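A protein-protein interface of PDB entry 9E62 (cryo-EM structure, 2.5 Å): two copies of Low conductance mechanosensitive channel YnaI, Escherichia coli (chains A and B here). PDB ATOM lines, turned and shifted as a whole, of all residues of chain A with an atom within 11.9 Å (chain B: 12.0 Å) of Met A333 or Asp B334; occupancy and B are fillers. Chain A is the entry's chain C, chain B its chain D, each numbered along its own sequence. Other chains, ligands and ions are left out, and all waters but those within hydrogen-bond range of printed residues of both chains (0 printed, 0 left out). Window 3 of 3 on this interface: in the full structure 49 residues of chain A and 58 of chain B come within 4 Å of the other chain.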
ATOM      1  N   GLN A 329      25.148  20.524  -9.101  1.00  0.00           N
ATOM      2  CA  GLN A 329      25.718  21.810  -8.736  1.00  0.00           C
ATOM      3  C   GLN A 329      24.889  22.431  -7.625  1.00  0.00           C
ATOM      4  O   GLN A 329      23.703  22.131  -7.474  1.00  0.00           O
ATOM      5  CB  GLN A 329      25.777  22.761  -9.935  1.00  0.00           C
ATOM      6  CG  GLN A 329      27.036  22.635 -10.767  1.00  0.00           C
ATOM      7  CD  GLN A 329      27.176  23.752 -11.774  1.00  0.00           C
ATOM      8  OE1 GLN A 329      28.196  24.438 -11.818  1.00  0.00           O
ATOM      9  NE2 GLN A 329      26.151  23.940 -12.593  1.00  0.00           N
ATOM     10  N   THR A 330      25.527  23.300  -6.848  1.00  0.00           N
ATOM     11  CA  THR A 330      24.860  24.094  -5.827  1.00  0.00           C
ATOM     12  C   THR A 330      24.918  25.552  -6.255  1.00  0.00           C
ATOM     13  O   THR A 330      26.002  26.081  -6.525  1.00  0.00           O
ATOM     14  CB  THR A 330      25.518  23.907  -4.459  1.00  0.00           C
ATOM     15  OG1 THR A 330      25.358  22.551  -4.032  1.00  0.00           O
ATOM     16  CG2 THR A 330      24.880  24.827  -3.435  1.00  0.00           C
ATOM     17  N   LEU A 331      23.762  26.199  -6.324  1.00  0.00           N
ATOM     18  CA  LEU A 331      23.656  27.561  -6.829  1.00  0.00           C
ATOM     19  C   LEU A 331      23.269  28.504  -5.702  1.00  0.00           C
ATOM     20  O   LEU A 331      22.288  28.260  -4.990  1.00  0.00           O
ATOM     21  CB  LEU A 331      22.634  27.645  -7.962  1.00  0.00           C
ATOM     22  CG  LEU A 331      22.827  26.648  -9.104  1.00  0.00           C
ATOM     23  CD1 LEU A 331      21.703  26.775 -10.114  1.00  0.00           C
ATOM     24  CD2 LEU A 331      24.175  26.846  -9.769  1.00  0.00           C
ATOM     25  N   TYR A 332      24.038  29.575  -5.544  1.00  0.00           N
ATOM     26  CA  TYR A 332      23.743  30.635  -4.588  1.00  0.00           C
ATOM     27  C   TYR A 332      23.267  31.853  -5.363  1.00  0.00           C
ATOM     28  O   TYR A 332      23.973  32.341  -6.250  1.00  0.00           O
ATOM     29  CB  TYR A 332      24.970  30.972  -3.744  1.00  0.00           C
ATOM     30  CG  TYR A 332      25.520  29.802  -2.966  1.00  0.00           C
ATOM     31  CD1 TYR A 332      25.026  29.486  -1.707  1.00  0.00           C
ATOM     32  CD2 TYR A 332      26.534  29.012  -3.487  1.00  0.00           C
ATOM     33  CE1 TYR A 332      25.524  28.419  -0.992  1.00  0.00           C
ATOM     34  CE2 TYR A 332      27.038  27.941  -2.776  1.00  0.00           C
ATOM     35  CZ  TYR A 332      26.530  27.650  -1.532  1.00  0.00           C
ATOM     36  OH  TYR A 332      27.029  26.584  -0.821  1.00  0.00           O
ATOM     37  N   MET A 333      22.078  32.340  -5.031  1.00  0.00           N
ATOM     38  CA  MET A 333      21.461  33.445  -5.750  1.00  0.00           C
ATOM     39  C   MET A 333      21.566  34.733  -4.945  1.00  0.00           C
ATOM     40  O   MET A 333      21.487  34.719  -3.713  1.00  0.00           O
ATOM     41  CB  MET A 333      19.996  33.144  -6.058  1.00  0.00           C
ATOM     42  CG  MET A 333      19.677  33.161  -7.533  1.00  0.00           C
ATOM     43  SD  MET A 333      20.038  31.597  -8.348  1.00  0.00           S
ATOM     44  CE  MET A 333      18.625  30.631  -7.834  1.00  0.00           C
ATOM     45  N   ASP A 334      21.746  35.841  -5.655  1.00  0.00           N
ATOM     46  CA  ASP A 334      21.841  37.158  -5.039  1.00  0.00           C
ATOM     47  C   ASP A 334      20.568  37.506  -4.275  1.00  0.00           C
ATOM     48  O   ASP A 334      20.454  38.589  -3.700  1.00  0.00           O
ATOM     49  CB  ASP A 334      22.120  38.221  -6.101  1.00  0.00           C
ATOM     50  CG  ASP A 334      21.079  38.231  -7.202  1.00  0.00           C
ATOM     51  OD1 ASP A 334      20.397  37.201  -7.388  1.00  0.00           O
ATOM     52  OD2 ASP A 334      20.939  39.268  -7.886  1.00  0.00           O
ATOM     53  N   THR B 330      21.495  18.441 -12.268  1.00  0.00           N
ATOM     54  CA  THR B 330      20.660  18.574 -11.083  1.00  0.00           C
ATOM     55  C   THR B 330      21.141  19.789 -10.304  1.00  0.00           C
ATOM     56  O   THR B 330      22.326  19.885  -9.968  1.00  0.00           O
ATOM     57  CB  THR B 330      20.723  17.317 -10.214  1.00  0.00           C
ATOM     58  OG1 THR B 330      20.168  16.211 -10.932  1.00  0.00           O
ATOM     59  CG2 THR B 330      19.936  17.519  -8.933  1.00  0.00           C
ATOM     60  N   LEU B 331      20.232  20.714 -10.022  1.00  0.00           N
ATOM     61  CA  LEU B 331      20.573  21.977  -9.386  1.00  0.00           C
ATOM     62  C   LEU B 331      19.982  22.031  -7.987  1.00  0.00           C
ATOM     63  O   LEU B 331      18.783  21.800  -7.805  1.00  0.00           O
ATOM     64  CB  LEU B 331      20.073  23.159 -10.215  1.00  0.00           C
ATOM     65  CG  LEU B 331      20.484  23.157 -11.688  1.00  0.00           C
ATOM     66  CD1 LEU B 331      19.853  24.328 -12.415  1.00  0.00           C
ATOM     67  CD2 LEU B 331      21.993  23.183 -11.826  1.00  0.00           C
ATOM     68  N   TYR B 332      20.825  22.335  -7.006  1.00  0.00           N
ATOM     69  CA  TYR B 332      20.402  22.539  -5.626  1.00  0.00           C
ATOM     70  C   TYR B 332      20.478  24.026  -5.322  1.00  0.00           C
ATOM     71  O   TYR B 332      21.539  24.640  -5.479  1.00  0.00           O
ATOM     72  CB  TYR B 332      21.273  21.740  -4.661  1.00  0.00           C
ATOM     73  CG  TYR B 332      21.271  20.253  -4.919  1.00  0.00           C
ATOM     74  CD1 TYR B 332      20.301  19.433  -4.359  1.00  0.00           C
ATOM     75  CD2 TYR B 332      22.240  19.667  -5.721  1.00  0.00           C
ATOM     76  CE1 TYR B 332      20.295  18.075  -4.592  1.00  0.00           C
ATOM     77  CE2 TYR B 332      22.240  18.308  -5.957  1.00  0.00           C
ATOM     78  CZ  TYR B 332      21.266  17.518  -5.392  1.00  0.00           C
ATOM     79  OH  TYR B 332      21.262  16.163  -5.625  1.00  0.00           O
ATOM     80  N   MET B 333      19.363  24.601  -4.891  1.00  0.00           N
ATOM     81  CA  MET B 333      19.271  26.033  -4.647  1.00  0.00           C
ATOM     82  C   MET B 333      19.310  26.329  -3.156  1.00  0.00           C
ATOM     83  O   MET B 333      18.783  25.561  -2.344  1.00  0.00           O
ATOM     84  CB  MET B 333      17.993  26.607  -5.255  1.00  0.00           C
ATOM     85  CG  MET B 333      18.246  27.688  -6.277  1.00  0.00           C
ATOM     86  SD  MET B 333      18.583  27.036  -7.921  1.00  0.00           S
ATOM     87  CE  MET B 333      16.927  26.623  -8.452  1.00  0.00           C
ATOM     88  N   ASP B 334      19.941  27.444  -2.806  1.00  0.00           N
ATOM     89  CA  ASP B 334      20.046  27.883  -1.420  1.00  0.00           C
ATOM     90  C   ASP B 334      18.670  28.123  -0.808  1.00  0.00           C
ATOM     91  O   ASP B 334      18.556  28.515   0.353  1.00  0.00           O
ATOM     92  CB  ASP B 334      20.888  29.155  -1.330  1.00  0.00           C
ATOM     93  CG  ASP B 334      20.345  30.275  -2.193  1.00  0.00           C
ATOM     94  OD1 ASP B 334      19.600  29.981  -3.152  1.00  0.00           O
ATOM     95  OD2 ASP B 334      20.661  31.452  -1.918  1.00  0.00           O
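The backbone carbonyl oxygen (O) of Thr B330 lies within hydrogen-bond range of the backbone NH (N) of Gln A329.
The backbone carbonyl oxygen (O) of Gln A329 lies within hydrogen-bond range of the backbone NH (N) of Tyr B332, at 2.9 Å.
O of Tyr B332 is in hydrogen-bond range of N of Leu A331 (2.8 Å).
The backbone carbonyl oxygen (O) of Leu A331 is in hydrogen-bond range of the backbone NH (N) of Asp B334 (3.3 Å).
Of the 6 printed residues of chain A, 4 touch a printed residue of chain B.
Printed residues of chain B that touch a printed residue of chain A: Thr B330, Leu B331, Tyr B332, Met B333 and Asp B334.
Among the printed residues, no Asp or Glu carboxylate lies within 4 Å of a Lys or Arg side-chain nitrogen of the other chain.
Printed residues of chain B within 4 Å of Gln A329: Thr B330, Leu B331 and Tyr B332.
Printed residues of chain B within 4 Å of Thr A330: Tyr B332 (3.4 Å).
Of chain B, only Leu B331 (3.8 Å), Tyr B332 (2.8 Å), Met B333 (3.8 Å) and Asp B334 (3.3 Å) come within 4 Å of Leu A331.
Of chain B, only Met B333 (3.4 Å) and Asp B334 (3.5 Å) come within 4 Å of Met A333.
No residue of chain B comes within 4 Å of Asp A334.
Printed residues of chain A within 4 Å of Leu B331: Gln A329 and Leu A331.
Printed residues of chain A within 4 Å of Tyr B332: Gln A329, Thr A330 and Leu A331.
Of chain A, only Leu A331 (3.8 Å) and Met A333 (3.4 Å) come within 4 Å of Met B333.
Printed residues of chain A within 4 Å of Asp B334: Leu A331 (3.3 Å) and Met A333 (3.5 Å).
The nearest residue of chain B that does not touch Met A333 is Tyr B332 (7.1 Å).
Thr A330 touches Tyr B332, but with the chains exchanged Tyr A332 does not touch Thr B330 (10.8 Å).
Leu A331 touches its own counterpart, Leu B331.
Leu A331 touches Met B333, but with the chains exchanged Met A333 does not touch Leu B331 (7.9 Å).
Leu A331 touches Asp B334, but with the chains exchanged Asp A334 does not touch Leu B331 (13.5 Å).
5 positions are printed for both chains.
Of the 10 pairs that touch across the chains among the printed residues, 2 have their exchanged pair printed and touching as well.
CA of Leu B331 touches O of Gln A329 (3.7 Å).
CA of Thr A330 touches O of Tyr B332, 3.4 Å away.
Leu A331 touches Leu B331 (CD1 to CD1, 3.8 Å).
Met B333 touches Leu A331 (CA to O, 3.8 Å).
Met B333 touches Met A333.
Met A333 touches Asp B334.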
